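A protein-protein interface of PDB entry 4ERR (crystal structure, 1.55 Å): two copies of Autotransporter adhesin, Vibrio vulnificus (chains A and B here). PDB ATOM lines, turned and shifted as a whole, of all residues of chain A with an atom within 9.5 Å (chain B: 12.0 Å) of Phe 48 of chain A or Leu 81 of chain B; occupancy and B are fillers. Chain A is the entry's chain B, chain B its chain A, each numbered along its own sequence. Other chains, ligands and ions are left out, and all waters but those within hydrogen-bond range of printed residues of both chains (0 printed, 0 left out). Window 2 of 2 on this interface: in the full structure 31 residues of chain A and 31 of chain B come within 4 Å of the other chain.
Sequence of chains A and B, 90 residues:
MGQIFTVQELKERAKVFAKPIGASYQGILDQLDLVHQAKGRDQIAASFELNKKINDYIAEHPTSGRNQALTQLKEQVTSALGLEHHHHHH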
ATOM      1  N   GLN A  31      25.946  18.624 -11.342  1.00  0.00           N
ATOM      2  CA  GLN A  31      24.603  18.667 -11.914  1.00  0.00           C
ATOM      3  C   GLN A  31      23.607  17.856 -11.078  1.00  0.00           C
ATOM      4  O   GLN A  31      22.429  18.247 -10.933  1.00  0.00           O
ATOM      5  CB  GLN A  31      24.627  18.162 -13.339  1.00  0.00           C
ATOM      6  CG  GLN A  31      23.315  18.356 -14.060  1.00  0.00           C
ATOM      7  CD  GLN A  31      22.966  19.823 -14.296  1.00  0.00           C
ATOM      8  OE1 GLN A  31      23.851  20.701 -14.411  1.00  0.00           O
ATOM      9  NE2 GLN A  31      21.668  20.098 -14.377  1.00  0.00           N
ATOM     10  N   VAL A  35      20.056  19.036  -9.399  1.00  0.00           N
ATOM     11  CA  VAL A  35      18.786  18.320  -9.475  1.00  0.00           C
ATOM     12  C   VAL A  35      18.127  18.286  -8.075  1.00  0.00           C
ATOM     13  O   VAL A  35      16.960  18.620  -7.927  1.00  0.00           O
ATOM     14  CB  VAL A  35      18.957  16.877 -10.040  1.00  0.00           C
ATOM     15  CG1 VAL A  35      17.677  16.076  -9.847  1.00  0.00           C
ATOM     16  CG2 VAL A  35      19.387  16.886 -11.546  1.00  0.00           C
ATOM     17  N   GLY A  40      10.233  21.884  -8.284  1.00  0.00           N
ATOM     18  CA  GLY A  40       9.316  21.945  -9.443  1.00  0.00           C
ATOM     19  C   GLY A  40       9.936  21.939 -10.837  1.00  0.00           C
ATOM     20  O   GLY A  40      10.762  21.078 -11.150  1.00  0.00           O
ATOM     21  N   ARG A  41       9.557  22.922 -11.655  1.00  0.00           N
ATOM     22  CA  ARG A  41      10.014  23.000 -13.056  1.00  0.00           C
ATOM     23  C   ARG A  41      11.532  23.012 -13.191  1.00  0.00           C
ATOM     24  O   ARG A  41      12.082  22.458 -14.150  1.00  0.00           O
ATOM     25  CB  ARG A  41       9.448  24.240 -13.762  1.00  0.00           C
ATOM     26  CG  ARG A  41       7.924  24.318 -13.825  1.00  0.00           C
ATOM     27  CD  ARG A  41       7.306  23.134 -14.577  1.00  0.00           C
ATOM     28  NE  ARG A  41       5.844  23.145 -14.496  1.00  0.00           N
ATOM     29  CZ  ARG A  41       5.062  22.122 -14.840  1.00  0.00           C
ATOM     30  NH1 ARG A  41       3.743  22.232 -14.721  1.00  0.00           N
ATOM     31  NH2 ARG A  41       5.588  20.986 -15.301  1.00  0.00           N
ATOM     32  N   ASP A  42      12.211  23.655 -12.245  1.00  0.00           N
ATOM     33  CA  ASP A  42      13.671  23.716 -12.277  1.00  0.00           C
ATOM     34  C   ASP A  42      14.272  22.305 -12.161  1.00  0.00           C
ATOM     35  O   ASP A  42      15.273  22.006 -12.821  1.00  0.00           O
ATOM     36  CB  ASP A  42      14.204  24.655 -11.185  1.00  0.00           C
ATOM     37  CG  ASP A  42      13.796  26.102 -11.410  1.00  0.00           C
ATOM     38  OD1 ASP A  42      13.193  26.395 -12.473  1.00  0.00           O
ATOM     39  OD2 ASP A  42      14.075  26.950 -10.530  1.00  0.00           O
ATOM     40  N   GLN A  43      13.639  21.434 -11.368  1.00  0.00           N
ATOM     41  CA  GLN A  43      14.130  20.062 -11.177  1.00  0.00           C
ATOM     42  C   GLN A  43      14.041  19.220 -12.465  1.00  0.00           C
ATOM     43  O   GLN A  43      14.938  18.415 -12.782  1.00  0.00           O
ATOM     44  CB  GLN A  43      13.386  19.391 -10.001  1.00  0.00           C
ATOM     45  CG  GLN A  43      13.960  18.083  -9.565  1.00  0.00           C
ATOM     46  CD  GLN A  43      13.473  17.657  -8.180  1.00  0.00           C
ATOM     47  OE1 GLN A  43      14.280  17.408  -7.274  1.00  0.00           O
ATOM     48  NE2 GLN A  43      12.160  17.593  -8.005  1.00  0.00           N
ATOM     49  N   ILE A  44      12.986  19.439 -13.238  1.00  0.00           N
ATOM     50  CA  ILE A  44      12.812  18.726 -14.506  1.00  0.00           C
ATOM     51  C   ILE A  44      13.921  19.090 -15.504  1.00  0.00           C
ATOM     52  O   ILE A  44      14.593  18.210 -16.088  1.00  0.00           O
ATOM     53  CB  ILE A  44      11.439  19.044 -15.149  1.00  0.00           C
ATOM     54  CG1 ILE A  44      10.310  18.471 -14.277  1.00  0.00           C
ATOM     55  CG2 ILE A  44      11.386  18.474 -16.578  1.00  0.00           C
ATOM     56  CD1 ILE A  44       8.915  18.991 -14.630  1.00  0.00           C
ATOM     57  N   ALA A  45      14.122  20.393 -15.700  1.00  0.00           N
ATOM     58  CA  ALA A  45      15.157  20.858 -16.613  1.00  0.00           C
ATOM     59  C   ALA A  45      16.540  20.330 -16.206  1.00  0.00           C
ATOM     60  O   ALA A  45      17.325  19.869 -17.050  1.00  0.00           O
ATOM     61  CB  ALA A  45      15.174  22.387 -16.696  1.00  0.00           C
ATOM     62  N   ALA A  46      16.828  20.373 -14.912  1.00  0.00           N
ATOM     63  CA  ALA A  46      18.127  19.950 -14.425  1.00  0.00           C
ATOM     64  C   ALA A  46      18.340  18.448 -14.685  1.00  0.00           C
ATOM     65  O   ALA A  46      19.476  18.012 -14.957  1.00  0.00           O
ATOM     66  CB  ALA A  46      18.265  20.273 -12.917  1.00  0.00           C
ATOM     67  N   SER A  47      17.254  17.669 -14.584  1.00  0.00           N
ATOM     68  CA  SER A  47      17.320  16.227 -14.784  1.00  0.00           C
ATOM     69  C   SER A  47      17.604  15.874 -16.232  1.00  0.00           C
ATOM     70  O   SER A  47      18.389  14.984 -16.509  1.00  0.00           O
ATOM     71  CB  SER A  47      16.037  15.551 -14.300  1.00  0.00           C
ATOM     72  OG  SER A  47      15.895  15.749 -12.908  1.00  0.00           O
ATOM     73  N   PHE A  48      17.010  16.611 -17.173  1.00  0.00           N
ATOM     74  CA  PHE A  48      17.366  16.396 -18.575  1.00  0.00           C
ATOM     75  C   PHE A  48      18.840  16.629 -18.835  1.00  0.00           C
ATOM     76  O   PHE A  48      19.489  15.872 -19.556  1.00  0.00           O
ATOM     77  CB  PHE A  48      16.546  17.291 -19.502  1.00  0.00           C
ATOM     78  CG  PHE A  48      15.189  16.737 -19.819  1.00  0.00           C
ATOM     79  CD1 PHE A  48      15.054  15.740 -20.778  1.00  0.00           C
ATOM     80  CD2 PHE A  48      14.052  17.176 -19.150  1.00  0.00           C
ATOM     81  CE1 PHE A  48      13.808  15.219 -21.094  1.00  0.00           C
ATOM     82  CE2 PHE A  48      12.772  16.645 -19.476  1.00  0.00           C
ATOM     83  CZ  PHE A  48      12.666  15.663 -20.435  1.00  0.00           C
ATOM     84  N   GLU A  49      19.388  17.683 -18.250  1.00  0.00           N
ATOM     85  CA  GLU A  49      20.783  17.980 -18.484  1.00  0.00           C
ATOM     86  C   GLU A  49      21.711  16.997 -17.786  1.00  0.00           C
ATOM     87  O   GLU A  49      22.785  16.686 -18.309  1.00  0.00           O
ATOM     88  CB  GLU A  49      21.124  19.420 -18.129  1.00  0.00           C
ATOM     89  CG  GLU A  49      22.274  19.911 -18.941  1.00  0.00           C
ATOM     90  CD  GLU A  49      21.952  20.035 -20.466  1.00  0.00           C
ATOM     91  OE1 GLU A  49      20.784  19.941 -20.891  1.00  0.00           O
ATOM     92  OE2 GLU A  49      22.870  20.242 -21.242  1.00  0.00           O
ATOM     93  N   LEU A  50      21.295  16.490 -16.628  1.00  0.00           N
ATOM     94  CA  LEU A  50      22.041  15.427 -15.963  1.00  0.00           C
ATOM     95  C   LEU A  50      22.133  14.194 -16.882  1.00  0.00           C
ATOM     96  O   LEU A  50      23.208  13.622 -17.072  1.00  0.00           O
ATOM     97  CB  LEU A  50      21.372  15.058 -14.639  1.00  0.00           C
ATOM     98  CG  LEU A  50      21.966  13.887 -13.878  1.00  0.00           C
ATOM     99  CD1 LEU A  50      23.417  14.145 -13.536  1.00  0.00           C
ATOM    100  CD2 LEU A  50      21.136  13.632 -12.631  1.00  0.00           C
ATOM    101  N   ASN A  51      21.004  13.808 -17.448  1.00  0.00           N
ATOM    102  CA  ASN A  51      20.979  12.663 -18.314  1.00  0.00           C
ATOM    103  C   ASN A  51      21.919  12.815 -19.518  1.00  0.00           C
ATOM    104  O   ASN A  51      22.637  11.876 -19.889  1.00  0.00           O
ATOM    105  CB  ASN A  51      19.555  12.321 -18.733  1.00  0.00           C
ATOM    106  CG  ASN A  51      19.330  10.842 -18.703  1.00  0.00           C
ATOM    107  OD1 ASN A  51      19.246  10.246 -17.627  1.00  0.00           O
ATOM    108  ND2 ASN A  51      19.288  10.227 -19.867  1.00  0.00           N
ATOM    109  N   LYS A  52      21.945  14.016 -20.101  1.00  0.00           N
ATOM    110  CA  LYS A  52      22.853  14.300 -21.183  1.00  0.00           C
ATOM    111  C   LYS A  52      24.306  14.167 -20.747  1.00  0.00           C
ATOM    112  O   LYS A  52      25.112  13.555 -21.458  1.00  0.00           O
ATOM    113  CB  LYS A  52      22.590  15.685 -21.780  1.00  0.00           C
ATOM    114  CG  LYS A  52      23.519  16.011 -22.882  1.00  0.00           C
ATOM    115  CD  LYS A  52      23.153  17.332 -23.587  1.00  0.00           C
ATOM    116  CE  LYS A  52      24.275  17.725 -24.521  1.00  0.00           C
ATOM    117  NZ  LYS A  52      24.743  16.617 -25.387  1.00  0.00           N
ATOM    118  N   LYS A  53      24.639  14.724 -19.584  1.00  0.00           N
ATOM    119  CA  LYS A  53      25.996  14.656 -19.074  1.00  0.00           C
ATOM    120  C   LYS A  53      26.431  13.198 -18.862  1.00  0.00           C
ATOM    121  O   LYS A  53      27.535  12.813 -19.248  1.00  0.00           O
ATOM    122  CB  LYS A  53      26.135  15.482 -17.785  1.00  0.00           C
ATOM    123  CG  LYS A  53      25.896  16.994 -17.992  1.00  0.00           C
ATOM    124  CD  LYS A  53      26.077  17.831 -16.720  1.00  0.00           C
ATOM    125  CE  LYS A  53      26.002  19.347 -17.021  1.00  0.00           C
ATOM    126  NZ  LYS A  53      27.141  19.872 -17.850  1.00  0.00           N
ATOM    127  N   ILE A  54      25.550  12.383 -18.287  1.00  0.00           N
ATOM    128  CA  ILE A  54      25.857  10.944 -18.063  1.00  0.00           C
ATOM    129  C   ILE A  54      26.066  10.261 -19.412  1.00  0.00           C
ATOM    130  O   ILE A  54      27.049   9.560 -19.607  1.00  0.00           O
ATOM    131  CB  ILE A  54      24.763  10.219 -17.277  1.00  0.00           C
ATOM    132  CG1 ILE A  54      24.597  10.845 -15.885  1.00  0.00           C
ATOM    133  CG2 ILE A  54      25.104   8.721 -17.161  1.00  0.00           C
ATOM    134  CD1 ILE A  54      23.349  10.408 -15.138  1.00  0.00           C
ATOM    135  N   ASN A  55      25.137  10.499 -20.332  1.00  0.00           N
ATOM    136  CA  ASN A  55      25.197   9.928 -21.678  1.00  0.00           C
ATOM    137  C   ASN A  55      26.529  10.267 -22.391  1.00  0.00           C
ATOM    138  O   ASN A  55      27.142   9.426 -23.041  1.00  0.00           O
ATOM    139  CB  ASN A  55      24.011  10.442 -22.488  1.00  0.00           C
ATOM    140  CG  ASN A  55      23.610   9.504 -23.595  1.00  0.00           C
ATOM    141  OD1 ASN A  55      23.480   8.284 -23.393  1.00  0.00           O
ATOM    142  ND2 ASN A  55      23.393  10.056 -24.773  1.00  0.00           N
ATOM    143  N   ASP A  56      26.944  11.523 -22.290  1.00  0.00           N
ATOM    144  CA  ASP A  56      28.183  11.999 -22.897  1.00  0.00           C
ATOM    145  C   ASP A  56      29.425  11.399 -22.229  1.00  0.00           C
ATOM    146  O   ASP A  56      30.386  11.038 -22.891  1.00  0.00           O
ATOM    147  CB  ASP A  56      28.238  13.510 -22.855  1.00  0.00           C
ATOM    148  CG  ASP A  56      27.195  14.172 -23.757  1.00  0.00           C
ATOM    149  OD1 ASP A  56      26.649  13.533 -24.686  1.00  0.00           O
ATOM    150  OD2 ASP A  56      26.918  15.362 -23.516  1.00  0.00           O
ATOM    151  N   GLY B   2      15.619   9.497  -1.834  1.00  0.00           N
ATOM    152  CA  GLY B   2      14.506   9.573  -2.826  1.00  0.00           C
ATOM    153  C   GLY B   2      14.741   8.617  -3.976  1.00  0.00           C
ATOM    154  O   GLY B   2      15.529   7.676  -3.850  1.00  0.00           O
ATOM    155  N   GLN B   3      14.106   8.882  -5.117  1.00  0.00           N
ATOM    156  CA  GLN B   3      14.221   7.972  -6.246  1.00  0.00           C
ATOM    157  C   GLN B   3      15.578   8.037  -6.956  1.00  0.00           C
ATOM    158  O   GLN B   3      16.107   6.998  -7.330  1.00  0.00           O
ATOM    159  CB  GLN B   3      13.062   8.098  -7.238  1.00  0.00           C
ATOM    160  CG  GLN B   3      13.362   8.713  -8.587  1.00  0.00           C
ATOM    161  CD  GLN B   3      12.848   7.807  -9.701  1.00  0.00           C
ATOM    162  OE1 GLN B   3      11.629   7.687  -9.926  1.00  0.00           O
ATOM    163  NE2 GLN B   3      13.781   7.120 -10.376  1.00  0.00           N
ATOM    164  N   ILE B   4      16.133   9.244  -7.097  1.00  0.00           N
ATOM    165  CA  ILE B   4      17.451   9.423  -7.715  1.00  0.00           C
ATOM    166  C   ILE B   4      18.510   9.493  -6.621  1.00  0.00           C
ATOM    167  O   ILE B   4      18.295  10.165  -5.614  1.00  0.00           O
ATOM    168  CB  ILE B   4      17.543  10.744  -8.523  1.00  0.00           C
ATOM    169  CG1 ILE B   4      16.396  10.839  -9.537  1.00  0.00           C
ATOM    170  CG2 ILE B   4      18.870  10.835  -9.237  1.00  0.00           C
ATOM    171  CD1 ILE B   4      16.298  12.191 -10.260  1.00  0.00           C
ATOM    172  N   PHE B   5      19.649   8.814  -6.809  1.00  0.00           N
ATOM    173  CA  PHE B   5      20.739   8.921  -5.844  1.00  0.00           C
ATOM    174  C   PHE B   5      21.044  10.382  -5.518  1.00  0.00           C
ATOM    175  O   PHE B   5      21.126  11.238  -6.428  1.00  0.00           O
ATOM    176  CB  PHE B   5      22.073   8.416  -6.422  1.00  0.00           C
ATOM    177  CG  PHE B   5      22.209   6.920  -6.607  1.00  0.00           C
ATOM    178  CD1 PHE B   5      21.842   6.007  -5.624  1.00  0.00           C
ATOM    179  CD2 PHE B   5      22.849   6.443  -7.755  1.00  0.00           C
ATOM    180  CE1 PHE B   5      22.052   4.661  -5.822  1.00  0.00           C
ATOM    181  CE2 PHE B   5      23.083   5.109  -7.944  1.00  0.00           C
ATOM    182  CZ  PHE B   5      22.688   4.218  -6.982  1.00  0.00           C
ATOM    183  N   GLN B  72      23.448   2.905 -13.279  1.00  0.00           N
ATOM    184  CA  GLN B  72      22.262   2.809 -12.433  1.00  0.00           C
ATOM    185  C   GLN B  72      21.632   4.203 -12.246  1.00  0.00           C
ATOM    186  O   GLN B  72      20.403   4.336 -12.306  1.00  0.00           O
ATOM    187  CB  GLN B  72      22.620   2.143 -11.118  1.00  0.00           C
ATOM    188  CG  GLN B  72      23.061   0.701 -11.328  1.00  0.00           C
ATOM    189  CD  GLN B  72      23.382   0.000 -10.041  1.00  0.00           C
ATOM    190  OE1 GLN B  72      24.045   0.570  -9.165  1.00  0.00           O
ATOM    191  NE2 GLN B  72      22.898  -1.237  -9.898  1.00  0.00           N
ATOM    192  N   LEU B  73      22.463   5.230 -12.010  1.00  0.00           N
ATOM    193  CA  LEU B  73      21.959   6.590 -11.894  1.00  0.00           C
ATOM    194  C   LEU B  73      21.161   6.996 -13.141  1.00  0.00           C
ATOM    195  O   LEU B  73      20.074   7.568 -13.020  1.00  0.00           O
ATOM    196  CB  LEU B  73      23.103   7.576 -11.648  1.00  0.00           C
ATOM    197  CG  LEU B  73      22.717   9.057 -11.611  1.00  0.00           C
ATOM    198  CD1 LEU B  73      21.770   9.381 -10.443  1.00  0.00           C
ATOM    199  CD2 LEU B  73      23.960   9.954 -11.589  1.00  0.00           C
ATOM    200  N   LYS B  74      21.659   6.685 -14.325  1.00  0.00           N
ATOM    201  CA  LYS B  74      20.930   7.060 -15.541  1.00  0.00           C
ATOM    202  C   LYS B  74      19.506   6.467 -15.505  1.00  0.00           C
ATOM    203  O   LYS B  74      18.498   7.199 -15.630  1.00  0.00           O
ATOM    204  CB  LYS B  74      21.698   6.601 -16.773  1.00  0.00           C
ATOM    205  CG  LYS B  74      21.288   7.283 -18.086  1.00  0.00           C
ATOM    206  CD  LYS B  74      22.188   6.825 -19.200  1.00  0.00           C
ATOM    207  CE  LYS B  74      21.547   7.012 -20.568  1.00  0.00           C
ATOM    208  NZ  LYS B  74      21.209   8.417 -20.810  1.00  0.00           N
ATOM    209  N   GLU B  75      19.407   5.154 -15.299  1.00  0.00           N
ATOM    210  CA  GLU B  75      18.082   4.550 -15.234  1.00  0.00           C
ATOM    211  C   GLU B  75      17.167   5.261 -14.237  1.00  0.00           C
ATOM    212  O   GLU B  75      15.994   5.440 -14.515  1.00  0.00           O
ATOM    213  CB  GLU B  75      18.125   3.043 -14.941  1.00  0.00           C
ATOM    214  CG  GLU B  75      18.019   2.180 -16.188  1.00  0.00           C
ATOM    215  CD  GLU B  75      16.875   2.622 -17.106  1.00  0.00           C
ATOM    216  OE1 GLU B  75      15.704   2.235 -16.874  1.00  0.00           O
ATOM    217  OE2 GLU B  75      17.151   3.351 -18.081  1.00  0.00           O
ATOM    218  N   GLN B  76      17.687   5.674 -13.083  1.00  0.00           N
ATOM    219  CA  GLN B  76      16.842   6.385 -12.111  1.00  0.00           C
ATOM    220  C   GLN B  76      16.350   7.690 -12.710  1.00  0.00           C
ATOM    221  O   GLN B  76      15.176   8.041 -12.575  1.00  0.00           O
ATOM    222  CB  GLN B  76      17.598   6.694 -10.823  1.00  0.00           C
ATOM    223  CG  GLN B  76      18.097   5.439 -10.109  1.00  0.00           C
ATOM    224  CD  GLN B  76      19.158   5.744  -9.096  1.00  0.00           C
ATOM    225  OE1 GLN B  76      19.592   6.896  -8.946  1.00  0.00           O
ATOM    226  NE2 GLN B  76      19.631   4.704  -8.426  1.00  0.00           N
ATOM    227  N   VAL B  77      17.258   8.407 -13.368  1.00  0.00           N
ATOM    228  CA  VAL B  77      16.883   9.681 -13.979  1.00  0.00           C
ATOM    229  C   VAL B  77      15.881   9.499 -15.126  1.00  0.00           C
ATOM    230  O   VAL B  77      14.911  10.251 -15.225  1.00  0.00           O
ATOM    231  CB  VAL B  77      18.101  10.458 -14.461  1.00  0.00           C
ATOM    232  CG1 VAL B  77      17.664  11.767 -15.172  1.00  0.00           C
ATOM    233  CG2 VAL B  77      18.990  10.756 -13.280  1.00  0.00           C
ATOM    234  N   THR B  78      16.157   8.546 -16.011  1.00  0.00           N
ATOM    235  CA  THR B  78      15.253   8.217 -17.121  1.00  0.00           C
ATOM    236  C   THR B  78      13.856   7.913 -16.617  1.00  0.00           C
ATOM    237  O   THR B  78      12.870   8.339 -17.220  1.00  0.00           O
ATOM    238  CB  THR B  78      15.774   7.008 -17.915  1.00  0.00           C
ATOM    239  OG1 THR B  78      16.977   7.384 -18.604  1.00  0.00           O
ATOM    240  CG2 THR B  78      14.745   6.518 -18.919  1.00  0.00           C
ATOM    241  N   SER B  79      13.762   7.160 -15.528  1.00  0.00           N
ATOM    242  CA  SER B  79      12.466   6.813 -14.961  1.00  0.00           C
ATOM    243  C   SER B  79      11.777   8.009 -14.310  1.00  0.00           C
ATOM    244  O   SER B  79      10.556   8.161 -14.408  1.00  0.00           O
ATOM    245  CB  SER B  79      12.629   5.672 -13.968  1.00  0.00           C
ATOM    246  OG  SER B  79      13.175   4.552 -14.634  1.00  0.00           O
ATOM    247  N   ALA B  80      12.565   8.871 -13.670  1.00  0.00           N
ATOM    248  CA  ALA B  80      12.049  10.087 -13.046  1.00  0.00           C
ATOM    249  C   ALA B  80      11.482  11.058 -14.101  1.00  0.00           C
ATOM    250  O   ALA B  80      10.561  11.843 -13.814  1.00  0.00           O
ATOM    251  CB  ALA B  80      13.152  10.762 -12.225  1.00  0.00           C
ATOM    252  N   LEU B  81      12.014  10.993 -15.323  1.00  0.00           N
ATOM    253  CA  LEU B  81      11.590  11.884 -16.405  1.00  0.00           C
ATOM    254  C   LEU B  81      10.475  11.274 -17.243  1.00  0.00           C
ATOM    255  O   LEU B  81       9.541  11.980 -17.623  1.00  0.00           O
ATOM    256  CB  LEU B  81      12.762  12.229 -17.336  1.00  0.00           C
ATOM    257  CG  LEU B  81      13.803  13.237 -16.846  1.00  0.00           C
ATOM    258  CD1 LEU B  81      15.044  13.190 -17.732  1.00  0.00           C
ATOM    259  CD2 LEU B  81      13.216  14.649 -16.792  1.00  0.00           C
ATOM    260  N   GLY B  82      10.595   9.974 -17.526  1.00  0.00           N
ATOM    261  CA  GLY B  82       9.697   9.252 -18.441  1.00  0.00           C
ATOM    262  C   GLY B  82      10.532   8.650 -19.572  1.00  0.00           C
ATOM    263  O   GLY B  82      11.747   8.885 -19.649  1.00  0.00           O
ATOM    264  N   LEU B  83       9.889   7.878 -20.447  1.00  0.00           N
ATOM    265  CA  LEU B  83      10.581   7.212 -21.569  1.00  0.00           C
ATOM    266  C   LEU B  83       9.588   6.620 -22.565  1.00  0.00           C
ATOM    267  O   LEU B  83       9.100   7.316 -23.452  1.00  0.00           O
ATOM    268  CB  LEU B  83      11.541   6.117 -21.043  1.00  0.00           C
ATOM    269  CG  LEU B  83      11.977   4.991 -22.003  1.00  0.00           C
ATOM    270  CD1 LEU B  83      12.473   5.525 -23.360  1.00  0.00           C
ATOM    271  CD2 LEU B  83      13.035   4.125 -21.340  1.00  0.00           C
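The side-chain amino group (NZ) of Lys 74 of chain B sits close to the side-chain amide nitrogen (ND2) of Asn 51 of chain A. The side-chain amino group (NZ) of Lys 74 of chain B is in hydrogen-bond range of the side-chain amide oxygen (OD1) of Asn 55 of chain A (3.4 Å).
Phe 48 of chain A touches one residue of chain B. Of the printed residues of chain A, Leu 81 of chain B touches Ile 44, Ser 47 and Phe 48. Ile 44 of chain A touches just one residue of chain B: Leu 81 (3.9 Å). No residue of chain B comes within 4 Å of Ala 46 of chain A. No residue of chain B comes within 4 Å of Lys 52 of chain A. No residue of chain A comes within 4 Å of Gly 82 of chain B. Printed residues of chain B within 4 Å of Asn 55 of chain A: Lys 74 (3.4 Å). Printed residues of chain B within 4 Å of Ile 54 of chain A: Leu 73 (3.6 Å). Of the printed residues of chain A, Leu 73 of chain B touches Ile 54. Printed residues of chain B within 4 Å of Asn 51 of chain A: Lys 74, Val 77 and Thr 78. Asp 56 of chain A touches none of the printed residues of chain B. Asp 42 of chain A touches none of the printed residues of chain B. The nearest residue of chain A that does not touch Leu 81 of chain B is Asn 51 of chain A (4.7 Å). The nearest printed residue of chain B that does not touch Ile 54 of chain A is Lys 74 of chain B (4.03 Å).
Hydrophobic or aromatic side chains of chain B that line the printed part of chain A: Leu 73, Val 77 and Leu 81. Hydrophobic or aromatic side chains of chain A within 4 Å of the printed part of chain B: Phe 48, Leu 50 and Ile 54. Among the printed residues, 10 pairs touch across the chains.
No position is printed for both chains.
CD2 of Leu 81 of chain B touches O of Ile 44 of chain A, 3.9 Å away. Ser 47 of chain A touches Val 77 of chain B. Ser 47 of chain A touches Leu 81 of chain B. Phe 48 of chain A touches Leu 81 of chain B (CE2 to CD2, 3.4 Å). CD2 of Leu 50 of chain A touches CG2 of Val 77 of chain B, at 3.6 Å. Asn 51 of chain A touches Val 77 of chain B (OD1 to CG1, 3.3 Å). Asn 51 of chain A touches Thr 78 of chain B. Leu 73 of chain B touches Ile 54 of chain A (CD2 to CD1, 3.6 Å).
The side-chain hydroxyl of Thr 78 of chain B lies within hydrogen-bond range of the backbone carbonyl oxygen of Lys 74 of chain B (3.3 Å). OG of Ser 47 of chain A is in hydrogen-bond range of O of Gln 43 of chain A, at 2.8 Å.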
